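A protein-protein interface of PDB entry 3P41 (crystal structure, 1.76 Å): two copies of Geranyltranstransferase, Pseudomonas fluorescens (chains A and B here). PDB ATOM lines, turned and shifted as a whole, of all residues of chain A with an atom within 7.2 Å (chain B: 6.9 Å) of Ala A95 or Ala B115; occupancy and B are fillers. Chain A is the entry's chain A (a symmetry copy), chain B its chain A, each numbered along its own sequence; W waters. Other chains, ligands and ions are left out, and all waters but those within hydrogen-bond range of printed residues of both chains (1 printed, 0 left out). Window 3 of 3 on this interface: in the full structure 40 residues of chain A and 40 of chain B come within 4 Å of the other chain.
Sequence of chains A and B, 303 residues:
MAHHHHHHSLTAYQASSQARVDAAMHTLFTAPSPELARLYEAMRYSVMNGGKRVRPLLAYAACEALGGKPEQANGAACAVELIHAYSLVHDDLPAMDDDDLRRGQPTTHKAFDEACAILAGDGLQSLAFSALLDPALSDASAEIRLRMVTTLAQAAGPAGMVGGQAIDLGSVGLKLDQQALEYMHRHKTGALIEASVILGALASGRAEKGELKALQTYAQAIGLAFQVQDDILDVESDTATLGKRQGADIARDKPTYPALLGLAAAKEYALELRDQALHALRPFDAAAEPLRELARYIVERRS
The side-chain carboxylate of Asp B113 is in hydrogen-bond range of N of SCY B116 (2.9 Å). O of Leu A93 sits at hydrogen-bond distance from N of Asp A98, 2.7 Å away.
Among the printed residues, merely in contact across the chains: His A90 with Ile B118, Leu A93 with Ile B118, Ala A95 with Glu B114, Ala A95 with Ala B115, Ala A95 with Ile B118, Met A96 with Ala B115, Leu A169 with Ala B115, Leu A169 with SCY B116 and Leu A169 with Leu B119.
Ala A95 touches just these residues of chain B: Glu B114, Ala B115 and Ile B118. Ala B115 touches just these residues of chain A: Ala A95, Met A96 and Leu A169. Printed residues of chain A within 4 Å of SCY B116: Leu A169. Printed residues of chain A within 4 Å of Glu B114: Ala A95. Of the printed residues of chain B, Leu A93 touches Ile B118 (3.9 Å). Of the printed residues of chain B, His A90 touches Ile B118. Of the printed residues of chain A, Leu B119 touches Leu A169 (3.6 Å). Asp A91 touches none of the printed residues of chain B. Phe B112 touches none of the printed residues of chain A.
Hydrophobic or aromatic side chains of chain B within 4 Å of the printed part of chain A: Ala B115, Ile B118 and Leu B119. Among the printed residues, 9 pairs touch across the chains. Among the printed residues, no Asp or Glu carboxylate lies within 4 Å of a Lys or Arg side-chain nitrogen of the other chain.
2 positions are printed for both chains. Of the 9 pairs that touch across the chains among the printed residues, none has its exchanged pair printed and touching as well.
Water W1 lies within hydrogen-bond range of the backbone NH (N) of Ala B115, the backbone carbonyl oxygen (O) of Ala A95 and the side-chain carboxylate (OD1) of Asp B113.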
ATOM      1  N   HIS A  90      22.020 -23.778  -2.537  1.00  0.00           N
ATOM      2  CA  HIS A  90      21.928 -23.946  -3.965  1.00  0.00           C
ATOM      3  C   HIS A  90      20.857 -23.057  -4.616  1.00  0.00           C
ATOM      4  O   HIS A  90      21.058 -22.609  -5.734  1.00  0.00           O
ATOM      5  CB  HIS A  90      21.640 -25.402  -4.258  1.00  0.00           C
ATOM      6  CG  HIS A  90      22.833 -26.270  -4.049  1.00  0.00           C
ATOM      7  ND1 HIS A  90      22.843 -27.613  -4.351  1.00  0.00           N
ATOM      8  CD2 HIS A  90      24.069 -25.969  -3.580  1.00  0.00           C
ATOM      9  CE1 HIS A  90      24.046 -28.102  -4.090  1.00  0.00           C
ATOM     10  NE2 HIS A  90      24.803 -27.130  -3.603  1.00  0.00           N
ATOM     11  N   ASP A  91      19.735 -22.858  -3.927  1.00  0.00           N
ATOM     12  CA  ASP A  91      18.647 -22.021  -4.493  1.00  0.00           C
ATOM     13  C   ASP A  91      19.119 -20.572  -4.774  1.00  0.00           C
ATOM     14  O   ASP A  91      18.775 -19.957  -5.796  1.00  0.00           O
ATOM     15  CB  ASP A  91      17.426 -22.042  -3.578  1.00  0.00           C
ATOM     16  CG  ASP A  91      16.305 -21.130  -4.069  1.00  0.00           C
ATOM     17  OD1 ASP A  91      15.470 -21.603  -4.855  1.00  0.00           O
ATOM     18  OD2 ASP A  91      16.246 -19.963  -3.646  1.00  0.00           O
ATOM     19  N   ASP A  92      19.923 -20.028  -3.876  1.00  0.00           N
ATOM     20  CA  ASP A  92      20.504 -18.701  -4.035  1.00  0.00           C
ATOM     21  C   ASP A  92      21.526 -18.574  -5.176  1.00  0.00           C
ATOM     22  O   ASP A  92      21.829 -17.452  -5.616  1.00  0.00           O
ATOM     23  CB  ASP A  92      21.128 -18.261  -2.695  1.00  0.00           C
ATOM     24  CG  ASP A  92      20.087 -17.983  -1.630  1.00  0.00           C
ATOM     25  OD1 ASP A  92      18.956 -17.605  -2.018  1.00  0.00           O
ATOM     26  OD2 ASP A  92      20.388 -18.141  -0.412  1.00  0.00           O
ATOM     27  N   LEU A  93      22.053 -19.690  -5.674  1.00  0.00           N
ATOM     28  CA  LEU A  93      23.170 -19.614  -6.653  1.00  0.00           C
ATOM     29  C   LEU A  93      22.810 -18.796  -7.891  1.00  0.00           C
ATOM     30  O   LEU A  93      21.635 -18.722  -8.274  1.00  0.00           O
ATOM     31  CB  LEU A  93      23.618 -20.996  -7.116  1.00  0.00           C
ATOM     32  CG  LEU A  93      24.288 -21.836  -6.045  1.00  0.00           C
ATOM     33  CD1 LEU A  93      24.550 -23.212  -6.620  1.00  0.00           C
ATOM     34  CD2 LEU A  93      25.562 -21.142  -5.633  1.00  0.00           C
ATOM     35  N   PRO A  94      23.817 -18.182  -8.517  1.00  0.00           N
ATOM     36  CA  PRO A  94      23.610 -17.380  -9.721  1.00  0.00           C
ATOM     37  C   PRO A  94      22.805 -18.089 -10.835  1.00  0.00           C
ATOM     38  O   PRO A  94      21.972 -17.449 -11.491  1.00  0.00           O
ATOM     39  CB  PRO A  94      25.040 -17.081 -10.181  1.00  0.00           C
ATOM     40  CG  PRO A  94      25.836 -17.058  -8.911  1.00  0.00           C
ATOM     41  CD  PRO A  94      25.232 -18.160  -8.078  1.00  0.00           C
ATOM     42  N   ALA A  95      23.037 -19.389 -11.030  1.00  0.00           N
ATOM     43  CA  ALA A  95      22.333 -20.168 -12.064  1.00  0.00           C
ATOM     44  C   ALA A  95      20.868 -20.410 -11.680  1.00  0.00           C
ATOM     45  O   ALA A  95      20.010 -20.654 -12.530  1.00  0.00           O
ATOM     46  CB  ALA A  95      23.045 -21.476 -12.297  1.00  0.00           C
ATOM     47  N   MET A  96      20.584 -20.308 -10.392  1.00  0.00           N
ATOM     48  CA  MET A  96      19.250 -20.552  -9.902  1.00  0.00           C
ATOM     49  C   MET A  96      18.603 -19.207  -9.705  1.00  0.00           C
ATOM     50  O   MET A  96      18.298 -18.523 -10.674  1.00  0.00           O
ATOM     51  CB  MET A  96      19.293 -21.318  -8.578  1.00  0.00           C
ATOM     52  CG  MET A  96      19.897 -22.704  -8.661  1.00  0.00           C
ATOM     53  SD  MET A  96      18.655 -24.056  -9.348  1.00  0.00           S
ATOM     54  CE  MET A  96      16.942 -23.385  -8.718  1.00  0.00           C
ATOM     55  N   ASP A  97      18.429 -18.791  -8.455  1.00  0.00           N
ATOM     56  CA  ASP A  97      17.760 -17.522  -8.180  1.00  0.00           C
ATOM     57  C   ASP A  97      18.693 -16.311  -8.198  1.00  0.00           C
ATOM     58  O   ASP A  97      18.231 -15.180  -8.268  1.00  0.00           O
ATOM     59  CB  ASP A  97      16.990 -17.602  -6.880  1.00  0.00           C
ATOM     60  CG  ASP A  97      15.795 -18.483  -7.006  1.00  0.00           C
ATOM     61  OD1 ASP A  97      15.127 -18.773  -5.990  1.00  0.00           O
ATOM     62  OD2 ASP A  97      15.538 -18.888  -8.160  1.00  0.00           O
ATOM     63  N   ASP A  98      20.004 -16.548  -8.155  1.00  0.00           N
ATOM     64  CA  ASP A  98      20.972 -15.441  -8.228  1.00  0.00           C
ATOM     65  C   ASP A  98      20.670 -14.339  -7.190  1.00  0.00           C
ATOM     66  O   ASP A  98      20.546 -13.153  -7.541  1.00  0.00           O
ATOM     67  CB  ASP A  98      21.022 -14.846  -9.651  1.00  0.00           C
ATOM     68  CG  ASP A  98      22.212 -13.893  -9.870  1.00  0.00           C
ATOM     69  OD1 ASP A  98      23.108 -13.821  -8.982  1.00  0.00           O
ATOM     70  OD2 ASP A  98      22.248 -13.217 -10.940  1.00  0.00           O
ATOM     71  N   GLU A 114      31.236 -19.158  -5.460  1.00  0.00           N
ATOM     72  CA  GLU A 114      30.259 -20.111  -6.002  1.00  0.00           C
ATOM     73  C   GLU A 114      30.636 -21.566  -5.787  1.00  0.00           C
ATOM     74  O   GLU A 114      29.788 -22.388  -5.423  1.00  0.00           O
ATOM     75  CB  GLU A 114      30.020 -19.859  -7.484  1.00  0.00           C
ATOM     76  CG  GLU A 114      28.663 -19.300  -7.772  1.00  0.00           C
ATOM     77  CD  GLU A 114      28.538 -18.825  -9.209  1.00  0.00           C
ATOM     78  OE1 GLU A 114      28.210 -19.648 -10.090  1.00  0.00           O
ATOM     79  OE2 GLU A 114      28.771 -17.624  -9.456  1.00  0.00           O
ATOM     80  N   LEU A 169      11.682 -24.234 -11.835  1.00  0.00           N
ATOM     81  CA  LEU A 169      12.418 -23.829 -13.051  1.00  0.00           C
ATOM     82  C   LEU A 169      11.597 -23.970 -14.324  1.00  0.00           C
ATOM     83  O   LEU A 169      11.580 -23.071 -15.168  1.00  0.00           O
ATOM     84  CB  LEU A 169      13.651 -24.694 -13.262  1.00  0.00           C
ATOM     85  CG  LEU A 169      14.868 -24.544 -12.372  1.00  0.00           C
ATOM     86  CD1 LEU A 169      15.868 -25.649 -12.743  1.00  0.00           C
ATOM     87  CD2 LEU A 169      15.464 -23.154 -12.546  1.00  0.00           C
ATOM     88  N   LEU B  93      30.595 -28.041 -13.479  1.00  0.00           N
ATOM     89  CA  LEU B  93      29.896 -26.729 -13.528  1.00  0.00           C
ATOM     90  C   LEU B  93      30.852 -25.562 -13.761  1.00  0.00           C
ATOM     91  O   LEU B  93      32.029 -25.630 -13.383  1.00  0.00           O
ATOM     92  CB  LEU B  93      29.115 -26.450 -12.248  1.00  0.00           C
ATOM     93  CG  LEU B  93      27.920 -27.358 -12.024  1.00  0.00           C
ATOM     94  CD1 LEU B  93      27.338 -27.044 -10.662  1.00  0.00           C
ATOM     95  CD2 LEU B  93      26.929 -27.110 -13.134  1.00  0.00           C
ATOM     96  N   HIS B 109      25.339 -29.607 -17.824  1.00  0.00           N
ATOM     97  CA  HIS B 109      24.996 -28.204 -17.856  1.00  0.00           C
ATOM     98  C   HIS B 109      25.082 -27.665 -19.288  1.00  0.00           C
ATOM     99  O   HIS B 109      24.512 -26.631 -19.578  1.00  0.00           O
ATOM    100  CB  HIS B 109      25.877 -27.388 -16.906  1.00  0.00           C
ATOM    101  CG  HIS B 109      27.324 -27.345 -17.303  1.00  0.00           C
ATOM    102  ND1 HIS B 109      27.861 -26.327 -18.065  1.00  0.00           N
ATOM    103  CD2 HIS B 109      28.345 -28.193 -17.036  1.00  0.00           C
ATOM    104  CE1 HIS B 109      29.152 -26.555 -18.249  1.00  0.00           C
ATOM    105  NE2 HIS B 109      29.467 -27.680 -17.640  1.00  0.00           N
ATOM    106  N   PHE B 112      21.729 -29.474 -20.962  1.00  0.00           N
ATOM    107  CA  PHE B 112      20.526 -28.920 -20.337  1.00  0.00           C
ATOM    108  C   PHE B 112      20.729 -27.425 -20.063  1.00  0.00           C
ATOM    109  O   PHE B 112      20.693 -26.611 -20.994  1.00  0.00           O
ATOM    110  CB  PHE B 112      20.116 -29.764 -19.100  1.00  0.00           C
ATOM    111  CG  PHE B 112      19.683 -31.186 -19.461  1.00  0.00           C
ATOM    112  CD1 PHE B 112      20.624 -32.159 -19.732  1.00  0.00           C
ATOM    113  CD2 PHE B 112      18.344 -31.518 -19.596  1.00  0.00           C
ATOM    114  CE1 PHE B 112      20.242 -33.449 -20.100  1.00  0.00           C
ATOM    115  CE2 PHE B 112      17.955 -32.789 -19.961  1.00  0.00           C
ATOM    116  CZ  PHE B 112      18.898 -33.764 -20.204  1.00  0.00           C
ATOM    117  N   ASP B 113      20.950 -27.057 -18.809  1.00  0.00           N
ATOM    118  CA  ASP B 113      21.436 -25.721 -18.463  1.00  0.00           C
ATOM    119  C   ASP B 113      21.998 -25.830 -17.061  1.00  0.00           C
ATOM    120  O   ASP B 113      21.948 -26.913 -16.485  1.00  0.00           O
ATOM    121  CB  ASP B 113      20.336 -24.655 -18.575  1.00  0.00           C
ATOM    122  CG  ASP B 113      19.276 -24.767 -17.499  1.00  0.00           C
ATOM    123  OD1 ASP B 113      18.529 -23.782 -17.315  1.00  0.00           O
ATOM    124  OD2 ASP B 113      19.175 -25.817 -16.838  1.00  0.00           O
ATOM    125  N   GLU B 114      22.561 -24.749 -16.526  1.00  0.00           N
ATOM    126  CA  GLU B 114      23.228 -24.828 -15.220  1.00  0.00           C
ATOM    127  C   GLU B 114      22.301 -25.203 -14.078  1.00  0.00           C
ATOM    128  O   GLU B 114      22.656 -26.025 -13.225  1.00  0.00           O
ATOM    129  CB  GLU B 114      23.936 -23.520 -14.894  1.00  0.00           C
ATOM    130  CG  GLU B 114      25.427 -23.633 -14.934  1.00  0.00           C
ATOM    131  CD  GLU B 114      26.103 -22.277 -14.855  1.00  0.00           C
ATOM    132  OE1 GLU B 114      26.332 -21.782 -13.731  1.00  0.00           O
ATOM    133  OE2 GLU B 114      26.403 -21.703 -15.923  1.00  0.00           O
ATOM    134  N   ALA B 115      21.117 -24.593 -14.058  1.00  0.00           N
ATOM    135  CA  ALA B 115      20.161 -24.814 -12.976  1.00  0.00           C
ATOM    136  C   ALA B 115      19.689 -26.258 -12.959  1.00  0.00           C
ATOM    137  O   ALA B 115      19.762 -26.946 -11.947  1.00  0.00           O
ATOM    138  CB  ALA B 115      18.972 -23.860 -13.121  1.00  0.00           C
ATOM    139  N   SCY B 116      19.401 -26.804 -14.173  1.00  0.00           N
ATOM    140  CA  SCY B 116      19.075 -28.196 -14.262  1.00  0.00           C
ATOM    141  CB  SCY B 116      18.837 -28.496 -15.735  1.00  0.00           C
ATOM    142  SG  SCY B 116      17.681 -29.802 -15.806  1.00  0.00           S
ATOM    143  CD  SCY B 116      16.237 -28.791 -15.626  1.00  0.00           C
ATOM    144  OCD SCY B 116      15.203 -29.248 -14.935  1.00  0.00           O
ATOM    145  CE  SCY B 116      16.238 -27.389 -16.229  1.00  0.00           C
ATOM    146  C   SCY B 116      20.224 -29.077 -13.796  1.00  0.00           C
ATOM    147  O   SCY B 116      19.939 -30.080 -13.162  1.00  0.00           O
ATOM    148  N   ALA B 117      21.376 -28.690 -14.241  1.00  0.00           N
ATOM    149  CA  ALA B 117      22.470 -29.605 -13.820  1.00  0.00           C
ATOM    150  C   ALA B 117      22.710 -29.604 -12.295  1.00  0.00           C
ATOM    151  O   ALA B 117      22.994 -30.652 -11.704  1.00  0.00           O
ATOM    152  CB  ALA B 117      23.743 -29.248 -14.557  1.00  0.00           C
ATOM    153  N   ILE B 118      22.659 -28.431 -11.667  1.00  0.00           N
ATOM    154  CA  ILE B 118      22.746 -28.378 -10.194  1.00  0.00           C
ATOM    155  C   ILE B 118      21.779 -29.324  -9.511  1.00  0.00           C
ATOM    156  O   ILE B 118      22.163 -30.146  -8.713  1.00  0.00           O
ATOM    157  CB  ILE B 118      22.526 -26.940  -9.674  1.00  0.00           C
ATOM    158  CG1 ILE B 118      23.709 -26.052 -10.094  1.00  0.00           C
ATOM    159  CG2 ILE B 118      22.287 -26.901  -8.143  1.00  0.00           C
ATOM    160  CD1 ILE B 118      23.386 -24.589 -10.103  1.00  0.00           C
ATOM    161  N   LEU B 119      20.492 -29.195  -9.828  1.00  0.00           N
ATOM    162  CA  LEU B 119      19.486 -30.076  -9.313  1.00  0.00           C
ATOM    163  C   LEU B 119      19.616 -31.546  -9.675  1.00  0.00           C
ATOM    164  O   LEU B 119      19.261 -32.379  -8.880  1.00  0.00           O
ATOM    165  CB  LEU B 119      18.134 -29.605  -9.836  1.00  0.00           C
ATOM    166  CG  LEU B 119      17.815 -28.218  -9.345  1.00  0.00           C
ATOM    167  CD1 LEU B 119      16.378 -27.811  -9.847  1.00  0.00           C
ATOM    168  CD2 LEU B 119      17.858 -28.163  -7.848  1.00  0.00           C
ATOM    169  N   ALA B 120      20.047 -31.846 -10.893  1.00  0.00           N
ATOM    170  CA  ALA B 120      20.225 -33.214 -11.292  1.00  0.00           C
ATOM    171  C   ALA B 120      21.241 -33.859 -10.353  1.00  0.00           C
ATOM    172  O   ALA B 120      21.015 -34.966  -9.915  1.00  0.00           O
ATOM    173  CB  ALA B 120      20.660 -33.330 -12.756  1.00  0.00           C
HETATM  174  O   HOH W   1      20.647 -21.838 -15.380  1.00  0.00           O
